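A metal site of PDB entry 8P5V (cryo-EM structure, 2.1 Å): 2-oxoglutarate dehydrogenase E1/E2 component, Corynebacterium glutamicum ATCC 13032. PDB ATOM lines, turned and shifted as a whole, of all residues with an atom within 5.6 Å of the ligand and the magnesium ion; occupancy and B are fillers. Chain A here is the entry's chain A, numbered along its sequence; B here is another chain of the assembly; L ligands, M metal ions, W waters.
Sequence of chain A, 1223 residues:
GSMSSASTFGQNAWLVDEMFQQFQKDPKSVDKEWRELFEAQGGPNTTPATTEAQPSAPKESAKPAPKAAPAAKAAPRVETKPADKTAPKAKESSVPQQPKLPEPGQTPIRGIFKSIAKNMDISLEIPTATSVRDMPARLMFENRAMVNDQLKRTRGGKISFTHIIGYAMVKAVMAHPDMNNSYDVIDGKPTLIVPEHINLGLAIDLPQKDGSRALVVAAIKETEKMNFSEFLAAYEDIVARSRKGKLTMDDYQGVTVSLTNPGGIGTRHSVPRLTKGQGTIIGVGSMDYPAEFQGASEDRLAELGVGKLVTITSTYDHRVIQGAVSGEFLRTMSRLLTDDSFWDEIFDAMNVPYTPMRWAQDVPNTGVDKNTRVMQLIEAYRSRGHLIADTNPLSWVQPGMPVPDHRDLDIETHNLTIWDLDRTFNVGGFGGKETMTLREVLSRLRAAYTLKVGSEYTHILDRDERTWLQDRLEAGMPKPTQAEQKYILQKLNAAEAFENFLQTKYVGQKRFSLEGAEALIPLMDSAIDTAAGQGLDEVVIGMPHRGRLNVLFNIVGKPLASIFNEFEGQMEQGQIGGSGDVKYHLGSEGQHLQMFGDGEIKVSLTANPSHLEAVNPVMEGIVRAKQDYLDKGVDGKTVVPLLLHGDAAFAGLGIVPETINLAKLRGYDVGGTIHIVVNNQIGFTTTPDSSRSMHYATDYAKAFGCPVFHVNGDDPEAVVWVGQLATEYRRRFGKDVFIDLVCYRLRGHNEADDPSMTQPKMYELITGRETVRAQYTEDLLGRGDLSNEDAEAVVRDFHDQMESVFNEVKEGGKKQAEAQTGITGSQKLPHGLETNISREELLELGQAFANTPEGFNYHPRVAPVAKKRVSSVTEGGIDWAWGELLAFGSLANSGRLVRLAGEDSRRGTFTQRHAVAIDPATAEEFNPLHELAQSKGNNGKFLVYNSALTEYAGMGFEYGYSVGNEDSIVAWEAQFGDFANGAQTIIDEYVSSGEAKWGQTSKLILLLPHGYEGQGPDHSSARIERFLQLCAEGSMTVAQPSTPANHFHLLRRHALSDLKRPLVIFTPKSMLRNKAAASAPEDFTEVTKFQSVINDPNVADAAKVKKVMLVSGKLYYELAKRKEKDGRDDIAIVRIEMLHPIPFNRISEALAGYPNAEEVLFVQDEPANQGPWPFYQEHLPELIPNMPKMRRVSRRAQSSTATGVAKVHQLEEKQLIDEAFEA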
ATOM      1  N   PHE A 512     -20.150 -16.969 -35.027  1.00  0.00           N
ATOM      2  CA  PHE A 512     -20.231 -15.508 -35.040  1.00  0.00           C
ATOM      3  C   PHE A 512     -19.360 -14.944 -36.163  1.00  0.00           C
ATOM      4  O   PHE A 512     -18.352 -14.305 -35.899  1.00  0.00           O
ATOM      5  CB  PHE A 512     -19.846 -14.918 -33.680  1.00  0.00           C
ATOM      6  CG  PHE A 512     -20.809 -15.235 -32.561  1.00  0.00           C
ATOM      7  CD1 PHE A 512     -22.108 -14.759 -32.610  1.00  0.00           C
ATOM      8  CD2 PHE A 512     -20.414 -16.005 -31.480  1.00  0.00           C
ATOM      9  CE1 PHE A 512     -23.008 -15.045 -31.587  1.00  0.00           C
ATOM     10  CE2 PHE A 512     -21.319 -16.295 -30.465  1.00  0.00           C
ATOM     11  CZ  PHE A 512     -22.610 -15.820 -30.520  1.00  0.00           C
ATOM     12  N   HIS A 545     -17.109 -11.406 -29.253  1.00  0.00           N
ATOM     13  CA  HIS A 545     -17.326 -12.612 -30.050  1.00  0.00           C
ATOM     14  C   HIS A 545     -17.174 -12.362 -31.553  1.00  0.00           C
ATOM     15  O   HIS A 545     -16.668 -13.209 -32.270  1.00  0.00           O
ATOM     16  CB  HIS A 545     -18.719 -13.166 -29.764  1.00  0.00           C
ATOM     17  CG  HIS A 545     -19.817 -12.179 -30.011  1.00  0.00           C
ATOM     18  ND1 HIS A 545     -20.735 -12.332 -31.034  1.00  0.00           N
ATOM     19  CD2 HIS A 545     -20.132 -11.010 -29.419  1.00  0.00           C
ATOM     20  CE1 HIS A 545     -21.562 -11.304 -31.034  1.00  0.00           C
ATOM     21  NE2 HIS A 545     -21.215 -10.481 -30.062  1.00  0.00           N
ATOM     22  N   ARG A 546     -17.648 -11.202 -32.033  1.00  0.00           N
ATOM     23  CA  ARG A 546     -17.828 -10.968 -33.455  1.00  0.00           C
ATOM     24  C   ARG A 546     -16.498 -11.080 -34.199  1.00  0.00           C
ATOM     25  O   ARG A 546     -15.662 -10.189 -34.122  1.00  0.00           O
ATOM     26  CB  ARG A 546     -18.461  -9.590 -33.687  1.00  0.00           C
ATOM     27  CG  ARG A 546     -18.785  -9.249 -35.139  1.00  0.00           C
ATOM     28  CD  ARG A 546     -19.792 -10.185 -35.776  1.00  0.00           C
ATOM     29  NE  ARG A 546     -21.058 -10.183 -35.053  1.00  0.00           N
ATOM     30  CZ  ARG A 546     -22.009 -11.100 -35.182  1.00  0.00           C
ATOM     31  NH1 ARG A 546     -21.903 -12.061 -36.072  1.00  0.00           N
ATOM     32  NH2 ARG A 546     -23.084 -11.034 -34.407  1.00  0.00           N
ATOM     33  N   SER A 610     -18.465 -14.110 -21.794  1.00  0.00           N
ATOM     34  CA  SER A 610     -19.518 -13.772 -22.733  1.00  0.00           C
ATOM     35  C   SER A 610     -20.144 -12.412 -22.393  1.00  0.00           C
ATOM     36  O   SER A 610     -20.820 -11.825 -23.227  1.00  0.00           O
ATOM     37  CB  SER A 610     -20.568 -14.845 -22.770  1.00  0.00           C
ATOM     38  OG  SER A 610     -21.538 -14.557 -23.768  1.00  0.00           O
ATOM     39  N   HIS A 611     -19.922 -11.928 -21.165  1.00  0.00           N
ATOM     40  CA  HIS A 611     -20.423 -10.642 -20.719  1.00  0.00           C
ATOM     41  C   HIS A 611     -19.707  -9.521 -21.473  1.00  0.00           C
ATOM     42  O   HIS A 611     -18.521  -9.292 -21.267  1.00  0.00           O
ATOM     43  CB  HIS A 611     -20.232 -10.491 -19.212  1.00  0.00           C
ATOM     44  CG  HIS A 611     -21.078 -11.412 -18.402  1.00  0.00           C
ATOM     45  ND1 HIS A 611     -21.306 -12.734 -18.722  1.00  0.00           N
ATOM     46  CD2 HIS A 611     -21.763 -11.177 -17.270  1.00  0.00           C
ATOM     47  CE1 HIS A 611     -22.107 -13.265 -17.815  1.00  0.00           C
ATOM     48  NE2 HIS A 611     -22.389 -12.341 -16.922  1.00  0.00           N
ATOM     49  N   LEU A 612     -20.452  -8.807 -22.322  1.00  0.00           N
ATOM     50  CA  LEU A 612     -19.873  -7.841 -23.241  1.00  0.00           C
ATOM     51  C   LEU A 612     -19.208  -6.694 -22.477  1.00  0.00           C
ATOM     52  O   LEU A 612     -19.699  -6.272 -21.443  1.00  0.00           O
ATOM     53  CB  LEU A 612     -20.980  -7.316 -24.172  1.00  0.00           C
ATOM     54  CG  LEU A 612     -21.573  -8.354 -25.129  1.00  0.00           C
ATOM     55  CD1 LEU A 612     -22.732  -7.758 -25.912  1.00  0.00           C
ATOM     56  CD2 LEU A 612     -20.517  -8.888 -26.085  1.00  0.00           C
ATOM     57  N   GLY A 646     -18.754  -3.913 -30.215  1.00  0.00           N
ATOM     58  CA  GLY A 646     -19.967  -3.860 -31.018  1.00  0.00           C
ATOM     59  C   GLY A 646     -20.730  -2.562 -30.775  1.00  0.00           C
ATOM     60  O   GLY A 646     -20.610  -1.981 -29.701  1.00  0.00           O
ATOM     61  N   ASP A 647     -21.504  -2.128 -31.775  1.00  0.00           N
ATOM     62  CA  ASP A 647     -22.184  -0.836 -31.717  1.00  0.00           C
ATOM     63  C   ASP A 647     -23.231  -0.824 -30.604  1.00  0.00           C
ATOM     64  O   ASP A 647     -23.318   0.153 -29.866  1.00  0.00           O
ATOM     65  CB  ASP A 647     -22.803  -0.454 -33.056  1.00  0.00           C
ATOM     66  CG  ASP A 647     -23.652  -1.528 -33.726  1.00  0.00           C
ATOM     67  OD1 ASP A 647     -23.470  -2.709 -33.390  1.00  0.00           O
ATOM     68  OD2 ASP A 647     -24.493  -1.166 -34.557  1.00  0.00           O
ATOM     69  N   ALA A 648     -24.019  -1.896 -30.488  1.00  0.00           N
ATOM     70  CA  ALA A 648     -25.052  -1.967 -29.460  1.00  0.00           C
ATOM     71  C   ALA A 648     -24.421  -1.965 -28.066  1.00  0.00           C
ATOM     72  O   ALA A 648     -24.881  -1.253 -27.184  1.00  0.00           O
ATOM     73  CB  ALA A 648     -25.931  -3.166 -29.659  1.00  0.00           C
ATOM     74  N   ALA A 649     -23.353  -2.755 -27.893  1.00  0.00           N
ATOM     75  CA  ALA A 649     -22.699  -2.876 -26.607  1.00  0.00           C
ATOM     76  C   ALA A 649     -21.980  -1.582 -26.248  1.00  0.00           C
ATOM     77  O   ALA A 649     -21.955  -1.189 -25.080  1.00  0.00           O
ATOM     78  CB  ALA A 649     -21.750  -4.047 -26.623  1.00  0.00           C
ATOM     79  N   PHE A 650     -21.370  -0.926 -27.245  1.00  0.00           N
ATOM     80  CA  PHE A 650     -20.603   0.282 -27.008  1.00  0.00           C
ATOM     81  C   PHE A 650     -21.537   1.383 -26.509  1.00  0.00           C
ATOM     82  O   PHE A 650     -21.177   2.122 -25.591  1.00  0.00           O
ATOM     83  CB  PHE A 650     -19.843   0.701 -28.264  1.00  0.00           C
ATOM     84  CG  PHE A 650     -18.885   1.850 -28.064  1.00  0.00           C
ATOM     85  CD1 PHE A 650     -19.308   3.171 -28.164  1.00  0.00           C
ATOM     86  CD2 PHE A 650     -17.566   1.616 -27.719  1.00  0.00           C
ATOM     87  CE1 PHE A 650     -18.426   4.218 -27.954  1.00  0.00           C
ATOM     88  CE2 PHE A 650     -16.684   2.663 -27.509  1.00  0.00           C
ATOM     89  CZ  PHE A 650     -17.113   3.962 -27.633  1.00  0.00           C
ATOM     90  N   LEU A 653     -23.944  -0.561 -22.896  1.00  0.00           N
ATOM     91  CA  LEU A 653     -23.323  -0.840 -21.612  1.00  0.00           C
ATOM     92  C   LEU A 653     -22.561   0.377 -21.109  1.00  0.00           C
ATOM     93  O   LEU A 653     -22.041   1.156 -21.904  1.00  0.00           O
ATOM     94  CB  LEU A 653     -22.398  -2.063 -21.744  1.00  0.00           C
ATOM     95  CG  LEU A 653     -23.097  -3.409 -21.902  1.00  0.00           C
ATOM     96  CD1 LEU A 653     -22.120  -4.478 -22.328  1.00  0.00           C
ATOM     97  CD2 LEU A 653     -23.824  -3.841 -20.621  1.00  0.00           C
ATOM     98  N   VAL A 678     -17.236  -1.964 -34.338  1.00  0.00           N
ATOM     99  CA  VAL A 678     -17.758  -2.669 -35.492  1.00  0.00           C
ATOM    100  C   VAL A 678     -19.241  -2.342 -35.588  1.00  0.00           C
ATOM    101  O   VAL A 678     -20.072  -3.004 -34.969  1.00  0.00           O
ATOM    102  CB  VAL A 678     -17.497  -4.183 -35.398  1.00  0.00           C
ATOM    103  CG1 VAL A 678     -18.030  -4.928 -36.617  1.00  0.00           C
ATOM    104  CG2 VAL A 678     -16.030  -4.486 -35.193  1.00  0.00           C
ATOM    105  N   ASN A 679     -19.556  -1.293 -36.358  1.00  0.00           N
ATOM    106  CA  ASN A 679     -20.915  -0.791 -36.463  1.00  0.00           C
ATOM    107  C   ASN A 679     -21.625  -1.521 -37.599  1.00  0.00           C
ATOM    108  O   ASN A 679     -21.669  -1.038 -38.721  1.00  0.00           O
ATOM    109  CB  ASN A 679     -20.893   0.730 -36.649  1.00  0.00           C
ATOM    110  CG  ASN A 679     -22.271   1.350 -36.660  1.00  0.00           C
ATOM    111  OD1 ASN A 679     -23.261   0.671 -36.388  1.00  0.00           O
ATOM    112  ND2 ASN A 679     -22.332   2.628 -36.966  1.00  0.00           N
ATOM    113  N   ASN A 680     -22.202  -2.692 -37.285  1.00  0.00           N
ATOM    114  CA  ASN A 680     -22.952  -3.466 -38.263  1.00  0.00           C
ATOM    115  C   ASN A 680     -24.435  -3.084 -38.211  1.00  0.00           C
ATOM    116  O   ASN A 680     -25.251  -3.745 -38.831  1.00  0.00           O
ATOM    117  CB  ASN A 680     -22.731  -4.970 -38.076  1.00  0.00           C
ATOM    118  CG  ASN A 680     -23.011  -5.447 -36.669  1.00  0.00           C
ATOM    119  OD1 ASN A 680     -23.495  -4.681 -35.831  1.00  0.00           O
ATOM    120  ND2 ASN A 680     -22.700  -6.698 -36.400  1.00  0.00           N
ATOM    121  N   GLN A 681     -24.745  -2.020 -37.458  1.00  0.00           N
ATOM    122  CA  GLN A 681     -26.032  -1.351 -37.512  1.00  0.00           C
ATOM    123  C   GLN A 681     -27.138  -2.240 -36.948  1.00  0.00           C
ATOM    124  O   GLN A 681     -28.305  -2.064 -37.315  1.00  0.00           O
ATOM    125  CB  GLN A 681     -26.348  -0.912 -38.949  1.00  0.00           C
ATOM    126  CG  GLN A 681     -25.259  -0.050 -39.568  1.00  0.00           C
ATOM    127  CD  GLN A 681     -25.587   0.358 -40.989  1.00  0.00           C
ATOM    128  OE1 GLN A 681     -26.499   1.145 -41.223  1.00  0.00           O
ATOM    129  NE2 GLN A 681     -24.821  -0.150 -41.939  1.00  0.00           N
ATOM    130  N   ILE A 682     -26.781  -3.161 -36.052  1.00  0.00           N
ATOM    131  CA  ILE A 682     -27.749  -4.064 -35.443  1.00  0.00           C
ATOM    132  C   ILE A 682     -27.113  -4.735 -34.229  1.00  0.00           C
ATOM    133  O   ILE A 682     -25.893  -4.895 -34.166  1.00  0.00           O
ATOM    134  CB  ILE A 682     -28.256  -5.098 -36.469  1.00  0.00           C
ATOM    135  CG1 ILE A 682     -29.537  -5.785 -35.985  1.00  0.00           C
ATOM    136  CG2 ILE A 682     -27.169  -6.110 -36.817  1.00  0.00           C
ATOM    137  CD1 ILE A 682     -30.213  -6.623 -37.050  1.00  0.00           C
ATOM    138  N   GLY A 683     -27.952  -5.111 -33.265  1.00  0.00           N
ATOM    139  CA  GLY A 683     -27.567  -5.963 -32.153  1.00  0.00           C
ATOM    140  C   GLY A 683     -27.873  -7.423 -32.466  1.00  0.00           C
ATOM    141  O   GLY A 683     -27.390  -7.975 -33.453  1.00  0.00           O
ATOM    142  N   PHE A 684     -28.685  -8.056 -31.612  1.00  0.00           N
ATOM    143  CA  PHE A 684     -29.230  -9.368 -31.881  1.00  0.00           C
ATOM    144  C   PHE A 684     -30.386  -9.194 -32.862  1.00  0.00           C
ATOM    145  O   PHE A 684     -30.319  -9.655 -33.999  1.00  0.00           O
ATOM    146  CB  PHE A 684     -29.616 -10.053 -30.571  1.00  0.00           C
ATOM    147  CG  PHE A 684     -29.944 -11.517 -30.639  1.00  0.00           C
ATOM    148  CD1 PHE A 684     -30.852 -12.016 -31.575  1.00  0.00           C
ATOM    149  CD2 PHE A 684     -29.379 -12.409 -29.737  1.00  0.00           C
ATOM    150  CE1 PHE A 684     -31.157 -13.368 -31.606  1.00  0.00           C
ATOM    151  CE2 PHE A 684     -29.684 -13.756 -29.785  1.00  0.00           C
ATOM    152  CZ  PHE A 684     -30.585 -14.237 -30.710  1.00  0.00           C
ATOM    153  N   ARG A 745     -24.089  -6.948 -41.008  1.00  0.00           N
ATOM    154  CA  ARG A 745     -24.021  -8.332 -40.569  1.00  0.00           C
ATOM    155  C   ARG A 745     -24.777  -9.186 -41.576  1.00  0.00           C
ATOM    156  O   ARG A 745     -26.006  -9.120 -41.642  1.00  0.00           O
ATOM    157  CB  ARG A 745     -24.613  -8.435 -39.164  1.00  0.00           C
ATOM    158  CG  ARG A 745     -24.413  -9.787 -38.493  1.00  0.00           C
ATOM    159  CD  ARG A 745     -25.370  -9.947 -37.325  1.00  0.00           C
ATOM    160  NE  ARG A 745     -26.752 -10.049 -37.787  1.00  0.00           N
ATOM    161  CZ  ARG A 745     -27.826  -9.857 -37.036  1.00  0.00           C
ATOM    162  NH1 ARG A 745     -27.719  -9.500 -35.767  1.00  0.00           N
ATOM    163  NH2 ARG A 745     -29.025 -10.032 -37.562  1.00  0.00           N
ATOM    164  N   HIS A 749     -27.749 -13.094 -36.039  1.00  0.00           N
ATOM    165  CA  HIS A 749     -26.853 -12.859 -34.925  1.00  0.00           C
ATOM    166  C   HIS A 749     -25.870 -14.018 -34.818  1.00  0.00           C
ATOM    167  O   HIS A 749     -24.661 -13.807 -34.745  1.00  0.00           O
ATOM    168  CB  HIS A 749     -27.649 -12.658 -33.630  1.00  0.00           C
ATOM    169  CG  HIS A 749     -26.775 -12.438 -32.447  1.00  0.00           C
ATOM    170  ND1 HIS A 749     -26.697 -13.344 -31.405  1.00  0.00           N
ATOM    171  CD2 HIS A 749     -25.923 -11.447 -32.150  1.00  0.00           C
ATOM    172  CE1 HIS A 749     -25.839 -12.887 -30.503  1.00  0.00           C
ATOM    173  NE2 HIS A 749     -25.359 -11.740 -30.940  1.00  0.00           N
ATOM    174  N   GLU B 903     -34.682  -7.987 -23.948  1.00  0.00           N
ATOM    175  CA  GLU B 903     -33.917  -8.074 -25.180  1.00  0.00           C
ATOM    176  C   GLU B 903     -34.563  -9.123 -26.090  1.00  0.00           C
ATOM    177  O   GLU B 903     -34.658 -10.296 -25.718  1.00  0.00           O
ATOM    178  CB  GLU B 903     -32.458  -8.396 -24.871  1.00  0.00           C
ATOM    179  CG  GLU B 903     -31.738  -7.269 -24.152  1.00  0.00           C
ATOM    180  CD  GLU B 903     -30.365  -7.625 -23.615  1.00  0.00           C
ATOM    181  OE1 GLU B 903     -29.937  -8.784 -23.806  1.00  0.00           O
ATOM    182  OE2 GLU B 903     -29.714  -6.741 -22.998  1.00  0.00           O
ATOM    183  N   ASP B 904     -35.040  -8.667 -27.246  1.00  0.00           N
ATOM    184  CA  ASP B 904     -35.569  -9.535 -28.290  1.00  0.00           C
ATOM    185  C   ASP B 904     -36.850 -10.223 -27.805  1.00  0.00           C
ATOM    186  O   ASP B 904     -37.101 -11.381 -28.143  1.00  0.00           O
ATOM    187  CB  ASP B 904     -34.514 -10.543 -28.743  1.00  0.00           C
ATOM    188  CG  ASP B 904     -33.174  -9.901 -29.075  1.00  0.00           C
ATOM    189  OD1 ASP B 904     -32.934  -9.639 -30.271  1.00  0.00           O
ATOM    190  OD2 ASP B 904     -32.382  -9.657 -28.141  1.00  0.00           O
ATOM    191  N   LEU B 949     -29.560  -2.849 -25.211  1.00  0.00           N
ATOM    192  CA  LEU B 949     -28.545  -3.775 -24.728  1.00  0.00           C
ATOM    193  C   LEU B 949     -28.132  -3.351 -23.325  1.00  0.00           C
ATOM    194  O   LEU B 949     -27.140  -2.636 -23.142  1.00  0.00           O
ATOM    195  CB  LEU B 949     -27.364  -3.727 -25.714  1.00  0.00           C
ATOM    196  CG  LEU B 949     -26.404  -4.925 -25.720  1.00  0.00           C
ATOM    197  CD1 LEU B 949     -25.694  -5.084 -24.381  1.00  0.00           C
ATOM    198  CD2 LEU B 949     -27.138  -6.201 -26.079  1.00  0.00           C
ATOM    199  N   GLU B 951     -28.891  -4.782 -18.970  1.00  0.00           N
ATOM    200  CA  GLU B 951     -29.593  -5.504 -17.917  1.00  0.00           C
ATOM    201  C   GLU B 951     -29.821  -4.575 -16.730  1.00  0.00           C
ATOM    202  O   GLU B 951     -30.916  -4.555 -16.178  1.00  0.00           O
ATOM    203  CB  GLU B 951     -28.799  -6.742 -17.489  1.00  0.00           C
ATOM    204  CG  GLU B 951     -28.814  -7.862 -18.510  1.00  0.00           C
ATOM    205  CD  GLU B 951     -27.933  -7.632 -19.722  1.00  0.00           C
ATOM    206  OE1 GLU B 951     -26.768  -7.219 -19.547  1.00  0.00           O
ATOM    207  OE2 GLU B 951     -28.409  -7.875 -20.854  1.00  0.00           O
ATOM    208  N   GLN B 975     -32.333 -12.338 -21.824  1.00  0.00           N
ATOM    209  CA  GLN B 975     -32.057 -13.154 -22.992  1.00  0.00           C
ATOM    210  C   GLN B 975     -31.615 -14.530 -22.518  1.00  0.00           C
ATOM    211  O   GLN B 975     -32.136 -15.547 -22.980  1.00  0.00           O
ATOM    212  CB  GLN B 975     -31.006 -12.468 -23.864  1.00  0.00           C
ATOM    213  CG  GLN B 975     -30.837 -13.145 -25.223  1.00  0.00           C
ATOM    214  CD  GLN B 975     -30.566 -12.133 -26.303  1.00  0.00           C
ATOM    215  OE1 GLN B 975     -29.631 -11.333 -26.201  1.00  0.00           O
ATOM    216  NE2 GLN B 975     -31.388 -12.134 -27.341  1.00  0.00           N
ATOM    217  N   PHE B 979     -27.024 -13.592 -17.742  1.00  0.00           N
ATOM    218  CA  PHE B 979     -26.674 -12.190 -17.891  1.00  0.00           C
ATOM    219  C   PHE B 979     -27.356 -11.318 -16.830  1.00  0.00           C
ATOM    220  O   PHE B 979     -27.068 -10.133 -16.749  1.00  0.00           O
ATOM    221  CB  PHE B 979     -27.039 -11.686 -19.289  1.00  0.00           C
ATOM    222  CG  PHE B 979     -26.370 -12.449 -20.410  1.00  0.00           C
ATOM    223  CD1 PHE B 979     -24.994 -12.589 -20.437  1.00  0.00           C
ATOM    224  CD2 PHE B 979     -27.118 -13.021 -21.421  1.00  0.00           C
ATOM    225  CE1 PHE B 979     -24.380 -13.302 -21.462  1.00  0.00           C
ATOM    226  CE2 PHE B 979     -26.504 -13.734 -22.446  1.00  0.00           C
ATOM    227  CZ  PHE B 979     -25.130 -13.870 -22.460  1.00  0.00           C
HETATM  228  N1  LIG L   1     -25.845  -8.765 -22.264  1.00  0.00           N
HETATM  229  C1  LIG L   1     -24.550  -8.892 -21.942  1.00  0.00           C
HETATM  230  C2  LIG L   1     -24.014  -7.983 -20.887  1.00  0.00           C
HETATM  231  N2  LIG L   1     -23.685  -9.756 -22.498  1.00  0.00           N
HETATM  232  C3  LIG L   1     -24.142 -10.570 -23.463  1.00  0.00           C
HETATM  233  N3  LIG L   1     -23.294 -11.486 -23.930  1.00  0.00           N
HETATM  234  C4  LIG L   1     -25.505 -10.506 -23.890  1.00  0.00           C
HETATM  235  C5  LIG L   1     -26.291  -9.587 -23.232  1.00  0.00           C
HETATM  236  C6  LIG L   1     -26.054 -11.347 -25.022  1.00  0.00           C
HETATM  237  N4  LIG L   1     -25.509 -10.947 -26.341  1.00  0.00           N
HETATM  238  C7  LIG L   1     -24.429 -11.460 -26.877  1.00  0.00           C
HETATM  239  S1  LIG L   1     -24.033 -10.737 -28.332  1.00  0.00           S
HETATM  240  C8  LIG L   1     -25.380  -9.693 -28.229  1.00  0.00           C
HETATM  241  C9  LIG L   1     -26.093  -9.929 -27.098  1.00  0.00           C
HETATM  242  C10 LIG L   1     -27.361  -9.278 -26.677  1.00  0.00           C
HETATM  243  C11 LIG L   1     -25.636  -8.650 -29.280  1.00  0.00           C
HETATM  244  C12 LIG L   1     -24.815  -7.394 -29.086  1.00  0.00           C
HETATM  245  O1  LIG L   1     -24.783  -6.664 -30.339  1.00  0.00           O
HETATM  246  P1  LIG L   1     -23.545  -5.721 -30.701  1.00  0.00           P
HETATM  247  O2  LIG L   1     -23.972  -4.715 -31.696  1.00  0.00           O
HETATM  248  O3  LIG L   1     -22.897  -5.245 -29.467  1.00  0.00           O
HETATM  249  O4  LIG L   1     -22.586  -6.790 -31.409  1.00  0.00           O
HETATM  250  P2  LIG L   1     -22.745  -7.645 -32.758  1.00  0.00           P
HETATM  251  O5  LIG L   1     -23.719  -6.898 -33.637  1.00  0.00           O
HETATM  252  O6  LIG L   1     -21.337  -7.672 -33.318  1.00  0.00           O
HETATM  253  O7  LIG L   1     -23.245  -9.016 -32.360  1.00  0.00           O
HETATM  254 MG    MG M   1     -23.901  -4.761 -33.850  1.00  0.00          MG
HETATM  255  O   HOH W   1     -20.457  -6.485 -29.007  1.00  0.00           O
HETATM  256  O   HOH W   2     -19.443  -7.509 -31.465  1.00  0.00           O
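Water W1 bridges O3 of the ligand (2.8 Å) and N of Gly 646 (3.3 Å).
O of Ile 682 binds the magnesium ion (2.0 Å).
OD1 of Asn 680 binds the magnesium ion.
The magnesium ion is bound by the side-chain carboxylate (OD1) of Asp 647 (2.1 Å).
O5 of the ligand is bound to the magnesium ion (2.2 Å).
The magnesium ion is bound by an oxygen (O2) of the ligand.
The magnesium ion has five donor atoms within binding distance.
Within 4 Å of the magnesium ion: Asp 647, Asn 680 and Ile 682.
O of Ser 610 lies within hydrogen-bond range of N3 of the ligand, at 2.6 Å.
A ring nitrogen (NE2) of His 749 lies close to a sulfur (S1) of the ligand (3.1 Å).
N2 of the ligand lies within hydrogen-bond range of N of Leu 612.
N of Ala 649 lies within hydrogen-bond range of O3 of the ligand (3.0 Å).
The guanidinium group (NH2) of Arg 546 lies within salt-bridge range of an oxygen (O7) of the ligand, 2.9 Å away.
A ring nitrogen (NE2) of His 545 lies close to a sulfur (S1) of the ligand, at 3.3 Å.
The backbone NH (N) of Ala 648 sits close to an oxygen (O2) of the ligand.
A nitrogen (N1) of the ligand sits close to the side-chain carboxylate (OE2) of Glu 951 of chain B, 3.1 Å away.
CA of His 611 touches N2 of the ligand, at 3.8 Å.
Gly 646 touches the ligand (CA to O3, 3.6 Å).
CA of Gly 683 touches O1 of the ligand, at 3.4 Å.
N of Phe 684 touches C11 of the ligand, at 3.9 Å.
OE1 of Glu 903 of chain B touches C5 of the ligand (3.8 Å).
CD2 of Leu 949 of chain B touches C10 of the ligand, 3.1 Å away.
OE1 of Gln 975 of chain B touches C10 of the ligand, at 3.1 Å.
Phe 979 of chain B touches the ligand.
Hydrophobic or aromatic side chains that line the ligand: His 545, Leu 612, Ala 648, Ala 649, His 749, Leu 949 of chain B and Phe 979 of chain B.
Of the 27 residues printed, 19 come within 4 Å of the ligand.
The backbone carbonyl oxygen (O) of Gly 683 lies within hydrogen-bond range of the guanidinium group (NH1) of Arg 745, 2.8 Å away.
O of Phe 684 sits at hydrogen-bond distance from NH1 of Arg 745 (3.1 Å).
The side-chain carboxylate (OD2) of Asp 904 of chain B sits at hydrogen-bond distance from the side-chain amide nitrogen (NE2) of Gln 975 of chain B (2.8 Å).
O of His 749 lies within hydrogen-bond range of NH2 of Arg 546 (3.2 Å).
The side-chain amide oxygen (OD1) of Asn 679 lies close to the side-chain carboxylate (OD2) of Asp 647 (2.9 Å).
The side-chain carboxylate (OD2) of Asp 647 sits at hydrogen-bond distance from the backbone NH (N) of Gln 681 (3.0 Å).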
